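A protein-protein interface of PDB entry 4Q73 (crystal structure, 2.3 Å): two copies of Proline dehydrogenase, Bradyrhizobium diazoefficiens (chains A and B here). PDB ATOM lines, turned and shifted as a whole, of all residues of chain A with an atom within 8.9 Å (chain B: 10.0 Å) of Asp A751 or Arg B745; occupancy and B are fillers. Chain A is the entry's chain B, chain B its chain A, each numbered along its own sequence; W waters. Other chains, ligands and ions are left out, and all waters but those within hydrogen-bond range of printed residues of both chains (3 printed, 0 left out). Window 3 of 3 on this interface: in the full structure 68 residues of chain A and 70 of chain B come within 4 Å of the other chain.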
ATOM      1  N   ALA A 724      -9.641   9.190  13.741  1.00  0.00           N
ATOM      2  CA  ALA A 724     -10.711   8.698  14.581  1.00  0.00           C
ATOM      3  C   ALA A 724     -11.048   7.262  14.185  1.00  0.00           C
ATOM      4  O   ALA A 724     -11.825   6.594  14.859  1.00  0.00           O
ATOM      5  CB  ALA A 724     -11.944   9.611  14.473  1.00  0.00           C
ATOM      6  N   PRO A 726     -11.062   3.494  14.045  1.00  0.00           N
ATOM      7  CA  PRO A 726     -10.738   2.529  15.108  1.00  0.00           C
ATOM      8  C   PRO A 726      -9.655   1.489  14.758  1.00  0.00           C
ATOM      9  O   PRO A 726      -9.104   0.877  15.682  1.00  0.00           O
ATOM     10  CB  PRO A 726     -12.083   1.828  15.361  1.00  0.00           C
ATOM     11  CG  PRO A 726     -12.823   1.951  14.058  1.00  0.00           C
ATOM     12  CD  PRO A 726     -12.438   3.318  13.543  1.00  0.00           C
ATOM     13  N   ARG A 741      -3.514  18.344  19.798  1.00  0.00           N
ATOM     14  CA  ARG A 741      -4.298  18.062  20.988  1.00  0.00           C
ATOM     15  C   ARG A 741      -5.634  17.443  20.631  1.00  0.00           C
ATOM     16  O   ARG A 741      -6.097  16.528  21.321  1.00  0.00           O
ATOM     17  CB  ARG A 741      -4.537  19.332  21.801  1.00  0.00           C
ATOM     18  CG  ARG A 741      -3.419  19.663  22.763  1.00  0.00           C
ATOM     19  CD  ARG A 741      -3.906  20.639  23.815  1.00  0.00           C
ATOM     20  NE  ARG A 741      -4.310  21.912  23.221  1.00  0.00           N
ATOM     21  CZ  ARG A 741      -3.479  22.929  23.015  1.00  0.00           C
ATOM     22  NH1 ARG A 741      -2.196  22.803  23.342  1.00  0.00           N
ATOM     23  NH2 ARG A 741      -3.925  24.055  22.465  1.00  0.00           N
ATOM     24  N   ASN A 744      -4.971  13.927  19.665  1.00  0.00           N
ATOM     25  CA  ASN A 744      -4.713  13.185  20.902  1.00  0.00           C
ATOM     26  C   ASN A 744      -6.006  12.887  21.665  1.00  0.00           C
ATOM     27  O   ASN A 744      -6.128  11.834  22.294  1.00  0.00           O
ATOM     28  CB  ASN A 744      -3.732  13.961  21.782  1.00  0.00           C
ATOM     29  CG  ASN A 744      -3.155  13.126  22.930  1.00  0.00           C
ATOM     30  OD1 ASN A 744      -2.910  11.918  22.800  1.00  0.00           O
ATOM     31  ND2 ASN A 744      -2.897  13.795  24.063  1.00  0.00           N
ATOM     32  N   ARG A 745      -6.984  13.791  21.578  1.00  0.00           N
ATOM     33  CA  ARG A 745      -8.263  13.601  22.276  1.00  0.00           C
ATOM     34  C   ARG A 745      -9.160  12.607  21.559  1.00  0.00           C
ATOM     35  O   ARG A 745      -9.881  11.828  22.191  1.00  0.00           O
ATOM     36  CB  ARG A 745      -8.996  14.938  22.428  1.00  0.00           C
ATOM     37  CG  ARG A 745      -8.472  15.762  23.590  1.00  0.00           C
ATOM     38  CD  ARG A 745      -8.716  17.241  23.414  1.00  0.00           C
ATOM     39  NE  ARG A 745      -7.983  17.985  24.433  1.00  0.00           N
ATOM     40  CZ  ARG A 745      -7.757  19.294  24.397  1.00  0.00           C
ATOM     41  NH1 ARG A 745      -7.053  19.866  25.371  1.00  0.00           N
ATOM     42  NH2 ARG A 745      -8.220  20.020  23.383  1.00  0.00           N
ATOM     43  N   ALA A 746      -9.126  12.660  20.232  1.00  0.00           N
ATOM     44  CA  ALA A 746      -9.860  11.703  19.419  1.00  0.00           C
ATOM     45  C   ALA A 746      -9.300  10.285  19.619  1.00  0.00           C
ATOM     46  O   ALA A 746     -10.064   9.317  19.656  1.00  0.00           O
ATOM     47  CB  ALA A 746      -9.820  12.104  17.953  1.00  0.00           C
ATOM     48  N   LEU A 747      -7.976  10.165  19.760  1.00  0.00           N
ATOM     49  CA  LEU A 747      -7.364   8.850  20.012  1.00  0.00           C
ATOM     50  C   LEU A 747      -7.762   8.321  21.388  1.00  0.00           C
ATOM     51  O   LEU A 747      -8.146   7.160  21.527  1.00  0.00           O
ATOM     52  CB  LEU A 747      -5.829   8.906  19.871  1.00  0.00           C
ATOM     53  CG  LEU A 747      -5.342   9.184  18.444  1.00  0.00           C
ATOM     54  CD1 LEU A 747      -3.867   9.548  18.379  1.00  0.00           C
ATOM     55  CD2 LEU A 747      -5.635   7.946  17.604  1.00  0.00           C
ATOM     56  N   ALA A 748      -7.723   9.183  22.398  1.00  0.00           N
ATOM     57  CA  ALA A 748      -7.978   8.736  23.758  1.00  0.00           C
ATOM     58  C   ALA A 748      -9.454   8.410  23.989  1.00  0.00           C
ATOM     59  O   ALA A 748      -9.803   7.636  24.884  1.00  0.00           O
ATOM     60  CB  ALA A 748      -7.500   9.787  24.751  1.00  0.00           C
ATOM     61  N   ALA A 749     -10.315   8.985  23.155  1.00  0.00           N
ATOM     62  CA  ALA A 749     -11.748   8.770  23.285  1.00  0.00           C
ATOM     63  C   ALA A 749     -12.124   7.350  22.879  1.00  0.00           C
ATOM     64  O   ALA A 749     -13.157   6.826  23.311  1.00  0.00           O
ATOM     65  CB  ALA A 749     -12.521   9.800  22.436  1.00  0.00           C
ATOM     66  N   LYS A 750     -11.294   6.730  22.037  1.00  0.00           N
ATOM     67  CA  LYS A 750     -11.560   5.371  21.550  1.00  0.00           C
ATOM     68  C   LYS A 750     -11.489   4.346  22.670  1.00  0.00           C
ATOM     69  O   LYS A 750     -10.697   4.492  23.611  1.00  0.00           O
ATOM     70  CB  LYS A 750     -10.563   4.981  20.466  1.00  0.00           C
ATOM     71  CG  LYS A 750     -10.569   5.837  19.218  1.00  0.00           C
ATOM     72  CD  LYS A 750      -9.478   5.333  18.283  1.00  0.00           C
ATOM     73  CE  LYS A 750      -9.222   6.281  17.110  1.00  0.00           C
ATOM     74  NZ  LYS A 750      -8.156   5.737  16.191  1.00  0.00           N
ATOM     75  N   ASP A 751     -12.303   3.298  22.572  1.00  0.00           N
ATOM     76  CA  ASP A 751     -12.250   2.241  23.570  1.00  0.00           C
ATOM     77  C   ASP A 751     -11.205   1.186  23.198  1.00  0.00           C
ATOM     78  O   ASP A 751     -10.903   0.288  23.988  1.00  0.00           O
ATOM     79  CB  ASP A 751     -13.633   1.628  23.769  1.00  0.00           C
ATOM     80  CG  ASP A 751     -14.543   2.528  24.590  1.00  0.00           C
ATOM     81  OD1 ASP A 751     -14.064   3.136  25.582  1.00  0.00           O
ATOM     82  OD2 ASP A 751     -15.732   2.641  24.233  1.00  0.00           O
ATOM     83  N   GLY A 752     -10.643   1.317  21.997  1.00  0.00           N
ATOM     84  CA  GLY A 752      -9.615   0.410  21.519  1.00  0.00           C
ATOM     85  C   GLY A 752      -8.268   0.549  22.206  1.00  0.00           C
ATOM     86  O   GLY A 752      -8.147   1.129  23.284  1.00  0.00           O
ATOM     87  N   PRO A 753      -7.220   0.013  21.570  1.00  0.00           N
ATOM     88  CA  PRO A 753      -5.867   0.160  22.129  1.00  0.00           C
ATOM     89  C   PRO A 753      -5.430   1.621  22.192  1.00  0.00           C
ATOM     90  O   PRO A 753      -5.872   2.431  21.354  1.00  0.00           O
ATOM     91  CB  PRO A 753      -4.994  -0.575  21.116  1.00  0.00           C
ATOM     92  CG  PRO A 753      -5.961  -1.546  20.405  1.00  0.00           C
ATOM     93  CD  PRO A 753      -7.257  -0.821  20.350  1.00  0.00           C
ATOM     94  N   ILE A 754      -4.616   1.944  23.204  1.00  0.00           N
ATOM     95  CA  ILE A 754      -3.939   3.238  23.305  1.00  0.00           C
ATOM     96  C   ILE A 754      -2.780   3.208  22.316  1.00  0.00           C
ATOM     97  O   ILE A 754      -1.841   2.434  22.478  1.00  0.00           O
ATOM     98  CB  ILE A 754      -3.431   3.496  24.754  1.00  0.00           C
ATOM     99  CG1 ILE A 754      -4.632   3.615  25.701  1.00  0.00           C
ATOM    100  CG2 ILE A 754      -2.524   4.766  24.842  1.00  0.00           C
ATOM    101  CD1 ILE A 754      -4.271   3.688  27.168  1.00  0.00           C
ATOM    102  N   ALA B 720      -6.385   9.629  40.366  1.00  0.00           N
ATOM    103  CA  ALA B 720      -6.911  10.530  39.344  1.00  0.00           C
ATOM    104  C   ALA B 720      -6.486  11.976  39.558  1.00  0.00           C
ATOM    105  O   ALA B 720      -6.264  12.709  38.594  1.00  0.00           O
ATOM    106  CB  ALA B 720      -8.428  10.441  39.292  1.00  0.00           C
ATOM    107  N   THR B 723      -2.898  12.204  38.166  1.00  0.00           N
ATOM    108  CA  THR B 723      -2.759  12.132  36.712  1.00  0.00           C
ATOM    109  C   THR B 723      -3.350  13.346  35.995  1.00  0.00           C
ATOM    110  O   THR B 723      -2.905  13.701  34.902  1.00  0.00           O
ATOM    111  CB  THR B 723      -3.377  10.842  36.149  1.00  0.00           C
ATOM    112  OG1 THR B 723      -4.797  10.849  36.369  1.00  0.00           O
ATOM    113  CG2 THR B 723      -2.791   9.652  36.857  1.00  0.00           C
ATOM    114  N   ALA B 724      -4.300  14.015  36.642  1.00  0.00           N
ATOM    115  CA  ALA B 724      -4.923  15.208  36.078  1.00  0.00           C
ATOM    116  C   ALA B 724      -4.134  16.472  36.430  1.00  0.00           C
ATOM    117  O   ALA B 724      -4.451  17.568  35.966  1.00  0.00           O
ATOM    118  CB  ALA B 724      -6.369  15.324  36.552  1.00  0.00           C
ATOM    119  N   VAL B 731       3.221   9.618  32.905  1.00  0.00           N
ATOM    120  CA  VAL B 731       2.622   8.587  33.737  1.00  0.00           C
ATOM    121  C   VAL B 731       3.092   7.177  33.359  1.00  0.00           C
ATOM    122  O   VAL B 731       3.076   6.773  32.189  1.00  0.00           O
ATOM    123  CB  VAL B 731       1.077   8.649  33.668  1.00  0.00           C
ATOM    124  CG1 VAL B 731       0.439   7.548  34.505  1.00  0.00           C
ATOM    125  CG2 VAL B 731       0.593  10.012  34.122  1.00  0.00           C
ATOM    126  N   THR B 737      -7.466  -2.280  32.097  1.00  0.00           N
ATOM    127  CA  THR B 737      -7.582  -1.606  30.816  1.00  0.00           C
ATOM    128  C   THR B 737      -8.468  -0.363  30.894  1.00  0.00           C
ATOM    129  O   THR B 737      -8.148   0.660  30.283  1.00  0.00           O
ATOM    130  CB  THR B 737      -8.089  -2.579  29.738  1.00  0.00           C
ATOM    131  OG1 THR B 737      -7.157  -3.659  29.621  1.00  0.00           O
ATOM    132  CG2 THR B 737      -8.177  -1.904  28.393  1.00  0.00           C
ATOM    133  N   GLU B 738      -9.536  -0.428  31.690  1.00  0.00           N
ATOM    134  CA  GLU B 738     -10.477   0.685  31.795  1.00  0.00           C
ATOM    135  C   GLU B 738      -9.833   1.900  32.463  1.00  0.00           C
ATOM    136  O   GLU B 738     -10.008   3.039  32.023  1.00  0.00           O
ATOM    137  CB  GLU B 738     -11.733   0.269  32.570  1.00  0.00           C
ATOM    138  N   VAL B 739      -9.080   1.649  33.527  1.00  0.00           N
ATOM    139  CA  VAL B 739      -8.408   2.719  34.250  1.00  0.00           C
ATOM    140  C   VAL B 739      -7.350   3.410  33.368  1.00  0.00           C
ATOM    141  O   VAL B 739      -7.233   4.640  33.371  1.00  0.00           O
ATOM    142  CB  VAL B 739      -7.797   2.184  35.570  1.00  0.00           C
ATOM    143  CG1 VAL B 739      -6.848   3.216  36.203  1.00  0.00           C
ATOM    144  CG2 VAL B 739      -8.921   1.804  36.546  1.00  0.00           C
ATOM    145  N   ALA B 740      -6.617   2.620  32.588  1.00  0.00           N
ATOM    146  CA  ALA B 740      -5.638   3.157  31.649  1.00  0.00           C
ATOM    147  C   ALA B 740      -6.267   4.108  30.635  1.00  0.00           C
ATOM    148  O   ALA B 740      -5.664   5.108  30.242  1.00  0.00           O
ATOM    149  CB  ALA B 740      -4.937   2.024  30.923  1.00  0.00           C
ATOM    150  N   ARG B 741      -7.468   3.778  30.183  1.00  0.00           N
ATOM    151  CA  ARG B 741      -8.162   4.626  29.225  1.00  0.00           C
ATOM    152  C   ARG B 741      -8.618   5.930  29.853  1.00  0.00           C
ATOM    153  O   ARG B 741      -8.563   6.995  29.223  1.00  0.00           O
ATOM    154  CB  ARG B 741      -9.346   3.882  28.612  1.00  0.00           C
ATOM    155  CG  ARG B 741      -8.941   2.997  27.435  1.00  0.00           C
ATOM    156  CD  ARG B 741     -10.151   2.686  26.601  1.00  0.00           C
ATOM    157  NE  ARG B 741     -11.129   1.925  27.368  1.00  0.00           N
ATOM    158  CZ  ARG B 741     -11.141   0.597  27.430  1.00  0.00           C
ATOM    159  NH1 ARG B 741     -10.230  -0.100  26.765  1.00  0.00           N
ATOM    160  NH2 ARG B 741     -12.059  -0.027  28.155  1.00  0.00           N
ATOM    161  N   SER B 742      -9.047   5.865  31.104  1.00  0.00           N
ATOM    162  CA  SER B 742      -9.510   7.080  31.753  1.00  0.00           C
ATOM    163  C   SER B 742      -8.314   7.994  32.067  1.00  0.00           C
ATOM    164  O   SER B 742      -8.422   9.216  31.971  1.00  0.00           O
ATOM    165  CB  SER B 742     -10.384   6.764  32.975  1.00  0.00           C
ATOM    166  OG  SER B 742      -9.617   6.421  34.106  1.00  0.00           O
ATOM    167  N   ILE B 743      -7.169   7.396  32.406  1.00  0.00           N
ATOM    168  CA  ILE B 743      -5.919   8.160  32.564  1.00  0.00           C
ATOM    169  C   ILE B 743      -5.515   8.803  31.239  1.00  0.00           C
ATOM    170  O   ILE B 743      -5.165   9.972  31.188  1.00  0.00           O
ATOM    171  CB  ILE B 743      -4.745   7.279  33.083  1.00  0.00           C
ATOM    172  CG1 ILE B 743      -4.932   6.957  34.565  1.00  0.00           C
ATOM    173  CG2 ILE B 743      -3.418   7.992  32.907  1.00  0.00           C
ATOM    174  CD1 ILE B 743      -4.039   5.834  35.053  1.00  0.00           C
ATOM    175  N   ASN B 744      -5.582   8.037  30.159  1.00  0.00           N
ATOM    176  CA  ASN B 744      -5.211   8.572  28.862  1.00  0.00           C
ATOM    177  C   ASN B 744      -6.116   9.735  28.483  1.00  0.00           C
ATOM    178  O   ASN B 744      -5.653  10.721  27.906  1.00  0.00           O
ATOM    179  CB  ASN B 744      -5.258   7.475  27.792  1.00  0.00           C
ATOM    180  CG  ASN B 744      -4.546   7.879  26.506  1.00  0.00           C
ATOM    181  OD1 ASN B 744      -3.523   8.572  26.536  1.00  0.00           O
ATOM    182  ND2 ASN B 744      -5.091   7.442  25.361  1.00  0.00           N
ATOM    183  N   ARG B 745      -7.386   9.654  28.882  1.00  0.00           N
ATOM    184  CA  ARG B 745      -8.351  10.695  28.537  1.00  0.00           C
ATOM    185  C   ARG B 745      -8.156  11.931  29.393  1.00  0.00           C
ATOM    186  O   ARG B 745      -8.260  13.059  28.900  1.00  0.00           O
ATOM    187  CB  ARG B 745      -9.785  10.184  28.706  1.00  0.00           C
ATOM    188  CG  ARG B 745     -10.249   9.297  27.557  1.00  0.00           C
ATOM    189  CD  ARG B 745     -11.402   8.379  27.930  1.00  0.00           C
ATOM    190  NE  ARG B 745     -11.615   7.431  26.837  1.00  0.00           N
ATOM    191  CZ  ARG B 745     -12.366   6.337  26.905  1.00  0.00           C
ATOM    192  NH1 ARG B 745     -12.467   5.555  25.836  1.00  0.00           N
ATOM    193  NH2 ARG B 745     -13.013   6.030  28.026  1.00  0.00           N
ATOM    194  N   ALA B 746      -7.851  11.711  30.670  1.00  0.00           N
ATOM    195  CA  ALA B 746      -7.572  12.816  31.578  1.00  0.00           C
ATOM    196  C   ALA B 746      -6.325  13.582  31.099  1.00  0.00           C
ATOM    197  O   ALA B 746      -6.307  14.806  31.120  1.00  0.00           O
ATOM    198  CB  ALA B 746      -7.394  12.299  33.005  1.00  0.00           C
ATOM    199  N   LEU B 747      -5.309  12.856  30.622  1.00  0.00           N
ATOM    200  CA  LEU B 747      -4.104  13.492  30.078  1.00  0.00           C
ATOM    201  C   LEU B 747      -4.399  14.242  28.782  1.00  0.00           C
ATOM    202  O   LEU B 747      -3.956  15.373  28.590  1.00  0.00           O
ATOM    203  CB  LEU B 747      -2.988  12.462  29.840  1.00  0.00           C
ATOM    204  CG  LEU B 747      -2.424  11.799  31.097  1.00  0.00           C
ATOM    205  CD1 LEU B 747      -1.607  10.544  30.754  1.00  0.00           C
ATOM    206  CD2 LEU B 747      -1.569  12.816  31.840  1.00  0.00           C
ATOM    207  N   ALA B 748      -5.174  13.626  27.901  1.00  0.00           N
ATOM    208  CA  ALA B 748      -5.388  14.221  26.592  1.00  0.00           C
ATOM    209  C   ALA B 748      -6.286  15.458  26.654  1.00  0.00           C
ATOM    210  O   ALA B 748      -6.236  16.300  25.754  1.00  0.00           O
ATOM    211  CB  ALA B 748      -5.959  13.189  25.628  1.00  0.00           C
ATOM    212  N   ALA B 749      -7.083  15.564  27.722  1.00  0.00           N
ATOM    213  CA  ALA B 749      -7.998  16.694  27.914  1.00  0.00           C
ATOM    214  C   ALA B 749      -7.243  17.974  28.264  1.00  0.00           C
ATOM    215  O   ALA B 749      -7.753  19.078  28.061  1.00  0.00           O
ATOM    216  CB  ALA B 749      -9.043  16.378  29.014  1.00  0.00           C
ATOM    217  N   LYS B 750      -6.039  17.821  28.811  1.00  0.00           N
ATOM    218  CA  LYS B 750      -5.230  18.959  29.243  1.00  0.00           C
ATOM    219  C   LYS B 750      -4.828  19.840  28.073  1.00  0.00           C
ATOM    220  O   LYS B 750      -4.624  19.344  26.960  1.00  0.00           O
ATOM    221  CB  LYS B 750      -3.967  18.482  29.952  1.00  0.00           C
ATOM    222  CG  LYS B 750      -4.205  17.644  31.187  1.00  0.00           C
ATOM    223  CD  LYS B 750      -2.861  17.235  31.775  1.00  0.00           C
ATOM    224  CE  LYS B 750      -3.000  16.223  32.895  1.00  0.00           C
ATOM    225  NZ  LYS B 750      -1.651  15.937  33.484  1.00  0.00           N
ATOM    226  N   ASP B 751      -4.711  21.145  28.327  1.00  0.00           N
ATOM    227  CA  ASP B 751      -4.271  22.063  27.291  1.00  0.00           C
ATOM    228  C   ASP B 751      -2.748  22.107  27.254  1.00  0.00           C
ATOM    229  O   ASP B 751      -2.154  22.631  26.311  1.00  0.00           O
ATOM    230  CB  ASP B 751      -4.829  23.471  27.520  1.00  0.00           C
ATOM    231  CG  ASP B 751      -6.296  23.593  27.145  1.00  0.00           C
ATOM    232  OD1 ASP B 751      -6.716  22.998  26.123  1.00  0.00           O
ATOM    233  OD2 ASP B 751      -7.022  24.316  27.863  1.00  0.00           O
ATOM    234  N   VAL B 755       1.961  14.426  27.291  1.00  0.00           N
ATOM    235  CA  VAL B 755       2.987  13.702  28.048  1.00  0.00           C
ATOM    236  C   VAL B 755       2.983  12.213  27.683  1.00  0.00           C
ATOM    237  O   VAL B 755       1.996  11.722  27.165  1.00  0.00           O
ATOM    238  CB  VAL B 755       2.815  13.917  29.575  1.00  0.00           C
ATOM    239  CG1 VAL B 755       2.885  15.441  29.924  1.00  0.00           C
ATOM    240  CG2 VAL B 755       1.514  13.310  30.057  1.00  0.00           C
ATOM    241  N   LEU B 757       2.466   8.283  27.983  1.00  0.00           N
ATOM    242  CA  LEU B 757       1.748   7.327  28.819  1.00  0.00           C
ATOM    243  C   LEU B 757       2.286   5.918  28.562  1.00  0.00           C
ATOM    244  O   LEU B 757       2.212   5.403  27.438  1.00  0.00           O
ATOM    245  CB  LEU B 757       0.222   7.371  28.578  1.00  0.00           C
ATOM    246  CG  LEU B 757      -0.588   6.321  29.351  1.00  0.00           C
ATOM    247  CD1 LEU B 757      -0.301   6.406  30.847  1.00  0.00           C
ATOM    248  CD2 LEU B 757      -2.107   6.416  29.108  1.00  0.00           C
ATOM    249  N   THR B 761      -1.358  -3.339  30.605  1.00  0.00           N
ATOM    250  CA  THR B 761      -2.692  -3.715  31.041  1.00  0.00           C
ATOM    251  C   THR B 761      -2.857  -5.244  30.942  1.00  0.00           C
ATOM    252  O   THR B 761      -1.860  -5.979  30.930  1.00  0.00           O
ATOM    253  CB  THR B 761      -3.790  -2.884  30.315  1.00  0.00           C
ATOM    254  OG1 THR B 761      -3.528  -2.859  28.911  1.00  0.00           O
ATOM    255  CG2 THR B 761      -3.777  -1.432  30.821  1.00  0.00           C
ATOM    256  N   THR B 912      -9.722 -11.079  20.217  1.00  0.00           N
ATOM    257  CA  THR B 912      -9.855 -10.493  21.548  1.00  0.00           C
ATOM    258  C   THR B 912      -9.288  -9.069  21.584  1.00  0.00           C
ATOM    259  O   THR B 912      -9.761  -8.218  22.348  1.00  0.00           O
ATOM    260  CB  THR B 912      -9.132 -11.330  22.616  1.00  0.00           C
ATOM    261  OG1 THR B 912      -7.716 -11.077  22.545  1.00  0.00           O
ATOM    262  CG2 THR B 912      -9.412 -12.839  22.430  1.00  0.00           C
ATOM    263  N   GLY B 913      -8.282  -8.818  20.749  1.00  0.00           N
ATOM    264  CA  GLY B 913      -7.622  -7.525  20.722  1.00  0.00           C
ATOM    265  C   GLY B 913      -6.484  -7.421  21.729  1.00  0.00           C
ATOM    266  O   GLY B 913      -5.747  -6.431  21.747  1.00  0.00           O
ATOM    267  N   TYR B 914      -6.366  -8.427  22.597  1.00  0.00           N
ATOM    268  CA  TYR B 914      -5.262  -8.504  23.551  1.00  0.00           C
ATOM    269  C   TYR B 914      -4.031  -9.149  22.918  1.00  0.00           C
ATOM    270  O   TYR B 914      -4.140  -9.801  21.880  1.00  0.00           O
ATOM    271  CB  TYR B 914      -5.676  -9.281  24.803  1.00  0.00           C
ATOM    272  CG  TYR B 914      -6.620  -8.522  25.710  1.00  0.00           C
ATOM    273  CD1 TYR B 914      -6.139  -7.633  26.669  1.00  0.00           C
ATOM    274  CD2 TYR B 914      -7.992  -8.706  25.613  1.00  0.00           C
ATOM    275  CE1 TYR B 914      -7.010  -6.943  27.504  1.00  0.00           C
ATOM    276  CE2 TYR B 914      -8.871  -8.024  26.439  1.00  0.00           C
ATOM    277  CZ  TYR B 914      -8.383  -7.151  27.380  1.00  0.00           C
ATOM    278  OH  TYR B 914      -9.273  -6.486  28.190  1.00  0.00           O
ATOM    279  N   GLY B 960      -1.643  -3.910  21.635  1.00  0.00           N
ATOM    280  CA  GLY B 960      -3.093  -3.886  21.512  1.00  0.00           C
ATOM    281  C   GLY B 960      -3.720  -3.495  22.835  1.00  0.00           C
ATOM    282  O   GLY B 960      -3.240  -2.565  23.467  1.00  0.00           O
ATOM    283  N   LEU B 961      -4.758  -4.210  23.280  1.00  0.00           N
ATOM    284  CA  LEU B 961      -5.366  -3.908  24.582  1.00  0.00           C
ATOM    285  C   LEU B 961      -4.437  -4.289  25.748  1.00  0.00           C
ATOM    286  O   LEU B 961      -4.714  -3.964  26.894  1.00  0.00           O
ATOM    287  CB  LEU B 961      -6.726  -4.609  24.739  1.00  0.00           C
ATOM    288  CG  LEU B 961      -7.819  -4.383  23.674  1.00  0.00           C
ATOM    289  CD1 LEU B 961      -9.065  -5.221  23.981  1.00  0.00           C
ATOM    290  CD2 LEU B 961      -8.201  -2.924  23.600  1.00  0.00           C
ATOM    291  N   SER B 962      -3.332  -4.970  25.458  1.00  0.00           N
ATOM    292  CA  SER B 962      -2.431  -5.407  26.523  1.00  0.00           C
ATOM    293  C   SER B 962      -1.431  -4.339  26.971  1.00  0.00           C
ATOM    294  O   SER B 962      -0.923  -4.401  28.089  1.00  0.00           O
ATOM    295  CB  SER B 962      -1.697  -6.696  26.128  1.00  0.00           C
ATOM    296  OG  SER B 962      -2.615  -7.776  26.032  1.00  0.00           O
HETATM  297  O   HOH W   1      -3.195  11.207  26.045  1.00  0.00           O
HETATM  298  O   HOH W   2      -4.104   9.526  23.383  1.00  0.00           O
HETATM  299  O   HOH W   3      -4.029  16.309  24.124  1.00  0.00           O
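Of the 28 printed residues of chain B, 11 touch a printed residue of chain A.
Along chain B the printed residues that touch a printed residue of chain A span positions 740 to 961.
Of the 14 printed residues of chain A, 10 touch a printed residue of chain B.
Hydrophobic or aromatic side chains of chain A within 4 Å of the printed part of chain B: Ala A748, Pro A753 and Ile A754.
Among the printed residues, 21 pairs touch across the chains.
Among the printed residues, Asp or Glu carboxylates within 4 Å of a Lys or Arg side-chain nitrogen of the other chain: Arg A741 with Asp B751 (3.9 Å), Arg A745 with Asp B751 (3.2 Å), Asp A751 with Arg B741 (3.6 Å) and Asp A751 with Arg B745 (2.9 Å).
Arg A741 touches Lys B750, and with the chains exchanged Lys A750 touches Arg B741.
Arg A741 touches Asp B751, and with the chains exchanged Asp A751 touches Arg B741.
Asn A744 touches Ala B748, and with the chains exchanged Ala A748 touches Asn B744.
Arg A745 touches Lys B750, and with the chains exchanged Lys A750 touches Arg B745.
The backbone carbonyl oxygen (O) of Thr B723 sits at hydrogen-bond distance from the side-chain amino group (NZ) of Lys B750 (2.9 Å).
OG1 of Thr B761 is in hydrogen-bond range of O of Leu B961, 2.6 Å away.
The backbone carbonyl oxygen of Gly B913 is in hydrogen-bond range of the backbone NH of Leu B961.
The guanidinium group (NE) of Arg B741 lies within salt-bridge range of the side-chain carboxylate (OD1) of Asp A751, at 3.6 Å.
The guanidinium group (NE) of Arg B745 lies within hydrogen-bond range of the backbone carbonyl oxygen (O) of Ala A748, 2.7 Å away.
NH1 of Arg B745 is in hydrogen-bond range of O of Ala A749, at 2.9 Å.
The guanidinium group (NH1) of Arg B745 sits at hydrogen-bond distance from the backbone carbonyl oxygen (O) of Lys A750 (3.0 Å).
The side-chain carboxylate of Asp A751 lies within salt-bridge range of the guanidinium group of Arg B745, 2.9 Å away.
NE of Arg A745 sits at hydrogen-bond distance from O of Ala B748 (2.8 Å).
The backbone carbonyl oxygen of Ala B749 sits at hydrogen-bond distance from the guanidinium group of Arg A745 (2.9 Å).
NH1 of Arg A745 lies within hydrogen-bond range of O of Lys B750 (2.9 Å).
The side-chain carboxylate (OD1) of Asp B751 is in salt-bridge range of the guanidinium group (NE) of Arg A741 (3.9 Å).
The guanidinium group (NH1) of Arg A745 lies within salt-bridge range of the side-chain carboxylate (OD1) of Asp B751 (3.2 Å).
Water W1 lies within hydrogen-bond range of the side-chain amide oxygen of Asn B744 (2.7 Å) and the side-chain amide nitrogen of Asn A744 (3.3 Å).
Water W2 lies within hydrogen-bond range of OD1 of Asn A744 (2.7 Å) and ND2 of Asn B744 (3.0 Å).
Water W3 lies within hydrogen-bond range of the backbone carbonyl oxygen of Ala B748, the side-chain amide nitrogen of Asn A744 and the backbone carbonyl oxygen of Arg A741.
Among the printed residues, pairs that only touch across the chains: Arg A741 with Lys B750, Asn A744 with Ala B748, Ala A748 with Asn B744, Ala A748 with Ala B748, Lys A750 with Arg B741, Gly A752 with Leu B961, Pro A753 with Gly B960, Pro A753 with Leu B961, Ile A754 with Ala B740, Ile A754 with Asn B744 and Ile A754 with Leu B757.
Of the printed residues of chain B, Arg A745 touches Ala B748, Ala B749, Lys B750 and Asp B751.
Of the printed residues of chain B, Ala A749 touches Arg B745 (2.9 Å).
Of the printed residues of chain B, Lys A750 touches Arg B741 and Arg B745.
Of chain B, only Arg B741 (2.9 Å) and Arg B745 (2.9 Å) come within 4 Å of Asp A751.
Gly A752 touches just one residue of chain B: Leu B961 (3.7 Å).
Arg B745 touches just these residues of chain A: Ala A748, Ala A749, Lys A750 and Asp A751.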
